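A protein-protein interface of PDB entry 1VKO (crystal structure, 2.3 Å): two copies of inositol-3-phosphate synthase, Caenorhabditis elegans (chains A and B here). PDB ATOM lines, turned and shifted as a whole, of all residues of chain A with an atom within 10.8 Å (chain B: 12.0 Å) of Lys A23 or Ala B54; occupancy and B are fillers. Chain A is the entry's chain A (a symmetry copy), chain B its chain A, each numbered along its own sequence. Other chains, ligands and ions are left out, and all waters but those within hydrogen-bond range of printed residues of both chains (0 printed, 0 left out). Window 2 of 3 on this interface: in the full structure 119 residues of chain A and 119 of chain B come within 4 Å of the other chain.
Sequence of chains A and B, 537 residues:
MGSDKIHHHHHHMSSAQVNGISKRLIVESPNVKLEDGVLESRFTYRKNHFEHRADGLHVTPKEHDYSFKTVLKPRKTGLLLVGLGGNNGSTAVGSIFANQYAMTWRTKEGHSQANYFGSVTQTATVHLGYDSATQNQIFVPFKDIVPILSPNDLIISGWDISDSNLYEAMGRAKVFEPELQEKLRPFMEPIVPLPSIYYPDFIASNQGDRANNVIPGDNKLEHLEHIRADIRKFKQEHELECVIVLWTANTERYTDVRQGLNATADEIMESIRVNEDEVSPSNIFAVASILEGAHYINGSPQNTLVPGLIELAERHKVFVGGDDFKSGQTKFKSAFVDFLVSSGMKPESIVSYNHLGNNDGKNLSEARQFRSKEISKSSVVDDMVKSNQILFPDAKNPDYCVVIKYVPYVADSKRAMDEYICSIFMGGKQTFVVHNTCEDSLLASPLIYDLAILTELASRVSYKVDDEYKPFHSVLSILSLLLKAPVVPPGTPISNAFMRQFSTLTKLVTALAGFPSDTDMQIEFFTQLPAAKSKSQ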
ATOM      1  N   LYS A  23       8.824  -6.029  -4.272  1.00  0.00           N
ATOM      2  CA  LYS A  23       7.495  -6.539  -3.823  1.00  0.00           C
ATOM      3  C   LYS A  23       7.618  -7.762  -2.892  1.00  0.00           C
ATOM      4  O   LYS A  23       7.717  -8.927  -3.322  1.00  0.00           O
ATOM      5  CB  LYS A  23       6.553  -6.797  -5.014  1.00  0.00           C
ATOM      6  CG  LYS A  23       5.840  -5.534  -5.532  1.00  0.00           C
ATOM      7  CD  LYS A  23       4.749  -5.855  -6.572  1.00  0.00           C
ATOM      8  N   ARG A  24       7.609  -7.471  -1.598  1.00  0.00           N
ATOM      9  CA  ARG A  24       7.685  -8.499  -0.590  1.00  0.00           C
ATOM     10  C   ARG A  24       6.281  -8.991  -0.171  1.00  0.00           C
ATOM     11  O   ARG A  24       5.277  -8.534  -0.701  1.00  0.00           O
ATOM     12  CB  ARG A  24       8.541  -8.006   0.594  1.00  0.00           C
ATOM     13  CG  ARG A  24       8.277  -6.572   1.034  1.00  0.00           C
ATOM     14  N   LEU A  25       6.227  -9.942   0.755  1.00  0.00           N
ATOM     15  CA  LEU A  25       4.982 -10.492   1.276  1.00  0.00           C
ATOM     16  C   LEU A  25       4.906 -10.000   2.725  1.00  0.00           C
ATOM     17  O   LEU A  25       5.774 -10.334   3.537  1.00  0.00           O
ATOM     18  CB  LEU A  25       5.055 -12.023   1.186  1.00  0.00           C
ATOM     19  CG  LEU A  25       3.936 -13.030   1.480  1.00  0.00           C
ATOM     20  CD1 LEU A  25       2.722 -12.802   0.620  1.00  0.00           C
ATOM     21  CD2 LEU A  25       4.433 -14.458   1.261  1.00  0.00           C
ATOM     22  N   ILE A  26       3.896  -9.178   3.035  1.00  0.00           N
ATOM     23  CA  ILE A  26       3.857  -8.383   4.287  1.00  0.00           C
ATOM     24  C   ILE A  26       2.696  -8.787   5.211  1.00  0.00           C
ATOM     25  O   ILE A  26       1.542  -8.783   4.794  1.00  0.00           O
ATOM     26  CB  ILE A  26       3.804  -6.867   3.961  1.00  0.00           C
ATOM     27  CG1 ILE A  26       4.924  -6.472   2.990  1.00  0.00           C
ATOM     28  CG2 ILE A  26       3.941  -6.015   5.226  1.00  0.00           C
ATOM     29  CD1 ILE A  26       4.599  -5.254   2.165  1.00  0.00           C
ATOM     30  N   VAL A  27       3.012  -9.154   6.457  1.00  0.00           N
ATOM     31  CA  VAL A  27       2.026  -9.673   7.409  1.00  0.00           C
ATOM     32  C   VAL A  27       1.340  -8.533   8.146  1.00  0.00           C
ATOM     33  O   VAL A  27       2.005  -7.591   8.563  1.00  0.00           O
ATOM     34  CB  VAL A  27       2.701 -10.436   8.567  1.00  0.00           C
ATOM     35  CG1 VAL A  27       1.729 -11.455   9.180  1.00  0.00           C
ATOM     36  CG2 VAL A  27       4.068 -11.018   8.167  1.00  0.00           C
ATOM     37  N   VAL A 140       2.022 -18.476  -3.137  1.00  0.00           N
ATOM     38  CA  VAL A 140       3.282 -17.755  -3.117  1.00  0.00           C
ATOM     39  C   VAL A 140       4.450 -18.723  -3.089  1.00  0.00           C
ATOM     40  O   VAL A 140       4.312 -19.860  -2.591  1.00  0.00           O
ATOM     41  CB  VAL A 140       3.407 -16.784  -1.925  1.00  0.00           C
ATOM     42  CG1 VAL A 140       2.343 -15.678  -2.019  1.00  0.00           C
ATOM     43  CG2 VAL A 140       3.390 -17.551  -0.592  1.00  0.00           C
ATOM     44  N   PRO A 141       5.578 -18.286  -3.644  1.00  0.00           N
ATOM     45  CA  PRO A 141       6.800 -19.052  -3.548  1.00  0.00           C
ATOM     46  C   PRO A 141       7.105 -19.329  -2.073  1.00  0.00           C
ATOM     47  O   PRO A 141       6.974 -18.440  -1.217  1.00  0.00           O
ATOM     48  CB  PRO A 141       7.857 -18.120  -4.170  1.00  0.00           C
ATOM     49  CG  PRO A 141       7.064 -17.242  -5.116  1.00  0.00           C
ATOM     50  CD  PRO A 141       5.759 -17.029  -4.407  1.00  0.00           C
ATOM     51  N   LYS A 143       9.907 -19.367  -0.854  1.00  0.00           N
ATOM     52  CA  LYS A 143      11.036 -18.556  -0.372  1.00  0.00           C
ATOM     53  C   LYS A 143      10.605 -17.136  -0.013  1.00  0.00           C
ATOM     54  O   LYS A 143      11.379 -16.390   0.555  1.00  0.00           O
ATOM     55  CB  LYS A 143      12.171 -18.541  -1.388  1.00  0.00           C
ATOM     56  CG  LYS A 143      11.782 -17.980  -2.764  1.00  0.00           C
ATOM     57  CD  LYS A 143      12.762 -18.465  -3.808  1.00  0.00           C
ATOM     58  CE  LYS A 143      12.308 -18.089  -5.181  1.00  0.00           C
ATOM     59  NZ  LYS A 143      12.496 -16.610  -5.250  1.00  0.00           N
ATOM     60  N   ASP A 144       9.354 -16.792  -0.332  1.00  0.00           N
ATOM     61  CA  ASP A 144       8.783 -15.505   0.014  1.00  0.00           C
ATOM     62  C   ASP A 144       8.151 -15.461   1.420  1.00  0.00           C
ATOM     63  O   ASP A 144       7.813 -14.392   1.914  1.00  0.00           O
ATOM     64  CB  ASP A 144       7.731 -15.117  -1.026  1.00  0.00           C
ATOM     65  CG  ASP A 144       8.337 -14.756  -2.375  1.00  0.00           C
ATOM     66  OD1 ASP A 144       9.556 -14.888  -2.564  1.00  0.00           O
ATOM     67  OD2 ASP A 144       7.658 -14.338  -3.325  1.00  0.00           O
ATOM     68  N   ILE A 145       7.970 -16.617   2.057  1.00  0.00           N
ATOM     69  CA  ILE A 145       7.264 -16.677   3.323  1.00  0.00           C
ATOM     70  C   ILE A 145       8.143 -16.245   4.504  1.00  0.00           C
ATOM     71  O   ILE A 145       7.855 -15.236   5.133  1.00  0.00           O
ATOM     72  CB  ILE A 145       6.639 -18.062   3.520  1.00  0.00           C
ATOM     73  CG1 ILE A 145       5.595 -18.313   2.441  1.00  0.00           C
ATOM     74  CG2 ILE A 145       6.003 -18.173   4.889  1.00  0.00           C
ATOM     75  CD1 ILE A 145       5.101 -19.782   2.428  1.00  0.00           C
ATOM     76  N   PHE B  50      -6.528 -10.568   1.842  1.00  0.00           N
ATOM     77  CA  PHE B  50      -5.411 -10.003   1.087  1.00  0.00           C
ATOM     78  C   PHE B  50      -5.641  -8.564   0.658  1.00  0.00           C
ATOM     79  O   PHE B  50      -6.779  -8.115   0.518  1.00  0.00           O
ATOM     80  CB  PHE B  50      -5.091 -10.888  -0.151  1.00  0.00           C
ATOM     81  CG  PHE B  50      -4.927 -12.339   0.181  1.00  0.00           C
ATOM     82  CD1 PHE B  50      -6.024 -13.199   0.166  1.00  0.00           C
ATOM     83  CD2 PHE B  50      -3.682 -12.844   0.549  1.00  0.00           C
ATOM     84  CE1 PHE B  50      -5.878 -14.552   0.521  1.00  0.00           C
ATOM     85  CE2 PHE B  50      -3.521 -14.203   0.890  1.00  0.00           C
ATOM     86  CZ  PHE B  50      -4.629 -15.054   0.880  1.00  0.00           C
ATOM     87  N   GLU B  51      -4.544  -7.847   0.448  1.00  0.00           N
ATOM     88  CA  GLU B  51      -4.599  -6.518  -0.135  1.00  0.00           C
ATOM     89  C   GLU B  51      -3.340  -6.284  -0.973  1.00  0.00           C
ATOM     90  O   GLU B  51      -2.218  -6.435  -0.485  1.00  0.00           O
ATOM     91  CB  GLU B  51      -4.725  -5.442   0.957  1.00  0.00           C
ATOM     92  CG  GLU B  51      -6.124  -5.258   1.544  1.00  0.00           C
ATOM     93  CD  GLU B  51      -6.195  -4.135   2.581  1.00  0.00           C
ATOM     94  OE1 GLU B  51      -5.542  -3.075   2.392  1.00  0.00           O
ATOM     95  OE2 GLU B  51      -6.918  -4.306   3.588  1.00  0.00           O
ATOM     96  N   HIS B  52      -3.531  -5.905  -2.232  1.00  0.00           N
ATOM     97  CA  HIS B  52      -2.416  -5.640  -3.133  1.00  0.00           C
ATOM     98  C   HIS B  52      -2.001  -4.171  -3.067  1.00  0.00           C
ATOM     99  O   HIS B  52      -2.824  -3.297  -3.233  1.00  0.00           O
ATOM    100  CB  HIS B  52      -2.763  -6.092  -4.542  1.00  0.00           C
ATOM    101  CG  HIS B  52      -3.350  -7.472  -4.583  1.00  0.00           C
ATOM    102  ND1 HIS B  52      -2.582  -8.605  -4.766  1.00  0.00           N
ATOM    103  CD2 HIS B  52      -4.625  -7.900  -4.426  1.00  0.00           C
ATOM    104  CE1 HIS B  52      -3.364  -9.671  -4.747  1.00  0.00           C
ATOM    105  NE2 HIS B  52      -4.607  -9.272  -4.533  1.00  0.00           N
ATOM    106  N   ARG B  53      -0.734  -3.915  -2.759  1.00  0.00           N
ATOM    107  CA  ARG B  53      -0.232  -2.561  -2.684  1.00  0.00           C
ATOM    108  C   ARG B  53       1.059  -2.472  -3.471  1.00  0.00           C
ATOM    109  O   ARG B  53       1.718  -3.494  -3.728  1.00  0.00           O
ATOM    110  CB  ARG B  53       0.010  -2.131  -1.234  1.00  0.00           C
ATOM    111  CG  ARG B  53      -1.234  -1.990  -0.319  1.00  0.00           C
ATOM    112  CD  ARG B  53      -2.275  -0.926  -0.732  1.00  0.00           C
ATOM    113  NE  ARG B  53      -3.522  -1.541  -1.221  1.00  0.00           N
ATOM    114  CZ  ARG B  53      -4.681  -1.591  -0.551  1.00  0.00           C
ATOM    115  NH1 ARG B  53      -4.784  -1.051   0.654  1.00  0.00           N
ATOM    116  NH2 ARG B  53      -5.745  -2.184  -1.094  1.00  0.00           N
ATOM    117  N   ALA B  54       1.399  -1.239  -3.848  1.00  0.00           N
ATOM    118  CA  ALA B  54       2.665  -0.891  -4.490  1.00  0.00           C
ATOM    119  C   ALA B  54       3.884  -1.674  -3.956  1.00  0.00           C
ATOM    120  O   ALA B  54       4.663  -2.220  -4.742  1.00  0.00           O
ATOM    121  CB  ALA B  54       2.901   0.629  -4.376  1.00  0.00           C
ATOM    122  N   ASP B  55       4.026  -1.747  -2.629  1.00  0.00           N
ATOM    123  CA  ASP B  55       5.179  -2.408  -1.978  1.00  0.00           C
ATOM    124  C   ASP B  55       5.083  -3.931  -1.824  1.00  0.00           C
ATOM    125  O   ASP B  55       6.065  -4.578  -1.478  1.00  0.00           O
ATOM    126  CB  ASP B  55       5.456  -1.766  -0.616  1.00  0.00           C
ATOM    127  CG  ASP B  55       4.272  -1.871   0.341  1.00  0.00           C
ATOM    128  OD1 ASP B  55       3.268  -2.548   0.013  1.00  0.00           O
ATOM    129  OD2 ASP B  55       4.271  -1.302   1.460  1.00  0.00           O
ATOM    130  N   GLY B  56       3.893  -4.486  -2.054  1.00  0.00           N
ATOM    131  CA  GLY B  56       3.693  -5.928  -2.185  1.00  0.00           C
ATOM    132  C   GLY B  56       2.351  -6.433  -1.674  1.00  0.00           C
ATOM    133  O   GLY B  56       1.366  -5.693  -1.632  1.00  0.00           O
ATOM    134  N   LEU B  57       2.324  -7.693  -1.248  1.00  0.00           N
ATOM    135  CA  LEU B  57       1.087  -8.354  -0.828  1.00  0.00           C
ATOM    136  C   LEU B  57       0.880  -8.377   0.684  1.00  0.00           C
ATOM    137  O   LEU B  57       1.663  -8.972   1.412  1.00  0.00           O
ATOM    138  CB  LEU B  57       1.099  -9.781  -1.343  1.00  0.00           C
ATOM    139  CG  LEU B  57      -0.184 -10.582  -1.322  1.00  0.00           C
ATOM    140  CD1 LEU B  57      -1.262  -9.865  -2.074  1.00  0.00           C
ATOM    141  CD2 LEU B  57       0.142 -11.887  -1.961  1.00  0.00           C
ATOM    142  N   HIS B  58      -0.195  -7.750   1.149  1.00  0.00           N
ATOM    143  CA  HIS B  58      -0.460  -7.686   2.575  1.00  0.00           C
ATOM    144  C   HIS B  58      -1.455  -8.760   2.958  1.00  0.00           C
ATOM    145  O   HIS B  58      -2.535  -8.851   2.371  1.00  0.00           O
ATOM    146  CB  HIS B  58      -0.952  -6.296   2.989  1.00  0.00           C
ATOM    147  CG  HIS B  58       0.056  -5.207   2.769  1.00  0.00           C
ATOM    148  ND1 HIS B  58       0.628  -4.503   3.806  1.00  0.00           N
ATOM    149  CD2 HIS B  58       0.598  -4.705   1.631  1.00  0.00           C
ATOM    150  CE1 HIS B  58       1.469  -3.607   3.319  1.00  0.00           C
ATOM    151  NE2 HIS B  58       1.470  -3.706   2.003  1.00  0.00           N
ATOM    152  N   VAL B  59      -1.064  -9.579   3.935  1.00  0.00           N
ATOM    153  CA  VAL B  59      -1.845 -10.731   4.372  1.00  0.00           C
ATOM    154  C   VAL B  59      -2.337 -10.525   5.797  1.00  0.00           C
ATOM    155  O   VAL B  59      -1.541 -10.414   6.716  1.00  0.00           O
ATOM    156  CB  VAL B  59      -1.031 -12.049   4.268  1.00  0.00           C
ATOM    157  CG1 VAL B  59      -1.930 -13.279   4.566  1.00  0.00           C
ATOM    158  CG2 VAL B  59      -0.365 -12.171   2.869  1.00  0.00           C
ATOM    159  N   GLN B 389       3.778 -20.033 -10.582  1.00  0.00           N
ATOM    160  CA  GLN B 389       4.301 -19.190 -11.659  1.00  0.00           C
ATOM    161  C   GLN B 389       5.819 -19.158 -11.808  1.00  0.00           C
ATOM    162  O   GLN B 389       6.315 -18.497 -12.710  1.00  0.00           O
ATOM    163  CB  GLN B 389       3.722 -17.786 -11.578  1.00  0.00           C
ATOM    164  CG  GLN B 389       2.454 -17.629 -12.402  1.00  0.00           C
ATOM    165  CD  GLN B 389       1.892 -16.224 -12.336  1.00  0.00           C
ATOM    166  OE1 GLN B 389       1.856 -15.611 -11.260  1.00  0.00           O
ATOM    167  NE2 GLN B 389       1.456 -15.704 -13.485  1.00  0.00           N
ATOM    168  N   ILE B 390       6.549 -19.866 -10.936  1.00  0.00           N
ATOM    169  CA  ILE B 390       7.989 -20.090 -11.143  1.00  0.00           C
ATOM    170  C   ILE B 390       8.118 -21.147 -12.245  1.00  0.00           C
ATOM    171  O   ILE B 390       8.750 -20.908 -13.284  1.00  0.00           O
ATOM    172  CB  ILE B 390       8.738 -20.527  -9.826  1.00  0.00           C
ATOM    173  CG1 ILE B 390       8.650 -19.441  -8.728  1.00  0.00           C
ATOM    174  CG2 ILE B 390      10.221 -20.905 -10.123  1.00  0.00           C
ATOM    175  CD1 ILE B 390       8.855 -19.974  -7.295  1.00  0.00           C
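O of Asp B55 is in hydrogen-bond range of N of Arg A24 (3.3 Å).
O of Leu B57 is in hydrogen-bond range of N of Ile A26, at 2.8 Å.
The backbone NH (N) of Val B59 is in hydrogen-bond range of the backbone carbonyl oxygen (O) of Ile A26, at 2.9 Å.
The backbone NH (N) of Leu B57 sits at hydrogen-bond distance from the backbone carbonyl oxygen (O) of Arg A24 (3.1 Å).
NE2 of His B58 is in hydrogen-bond range of OD1 of Asp B55 (2.9 Å).
The backbone NH of His B58 lies within hydrogen-bond range of the backbone carbonyl oxygen of Glu B51, 2.9 Å away.
CG of Lys A23 touches O of Ala B54 (3.6 Å).
Asp B55 touches Lys A23 (O to CA, 3.4 Å).
Gly B56 touches Lys A23 (CA to CG, 3.996 Å).
Gly B56 touches Arg A24.
C of Leu A25 touches O of Leu B57, at 3.6 Å.
Leu A25 touches Val B59 (CD1 to CG2, 3.9 Å).
Asp B55 touches Ile A26 (OD1 to CD1, 3.7 Å).
His B58 touches Ile A26.
Val B59 touches Val A27 (O to CA, 3.7 Å).
CD1 of Ile B390 touches CB of Pro A141, at 3.8 Å.
Ala B54 touches one residue of chain A.
Printed residues of chain B within 4 Å of Val A27: Val B59.
Of the printed residues of chain A, Gly B56 touches Lys A23 (3.996 Å) and Arg A24 (3.4 Å).
Printed residues of chain B within 4 Å of Ile A26: Asp B55, Leu B57, His B58 and Val B59.
Printed residues of chain A within 4 Å of His B58: Ile A26 (3.2 Å).
Printed residues of chain B within 4 Å of Pro A141: Ile B390.
Ile A145 touches none of the printed residues of chain B.
Arg B53 touches none of the printed residues of chain A.
The nearest residue of chain A that does not touch Ala B54 is Arg A24 (6.8 Å).
The nearest printed residue of chain A that does not touch Val B59 is Val A140 (6.6 Å).
Of the 10 printed residues of chain A, 6 touch a printed residue of chain B.
Printed residues of chain A that touch a printed residue of chain B: Lys A23, Arg A24, Leu A25, Ile A26, Val A27 and Pro A141.
Of the 12 printed residues of chain B, 7 touch a printed residue of chain A.
Printed residues of chain B that touch a printed residue of chain A: Ala B54, Asp B55, Gly B56, Leu B57, His B58, Val B59 and Ile B390.
No position is printed for both chains.
Of the 14 pairs that touch across the chains among the printed residues, none has its exchanged pair printed and touching as well.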
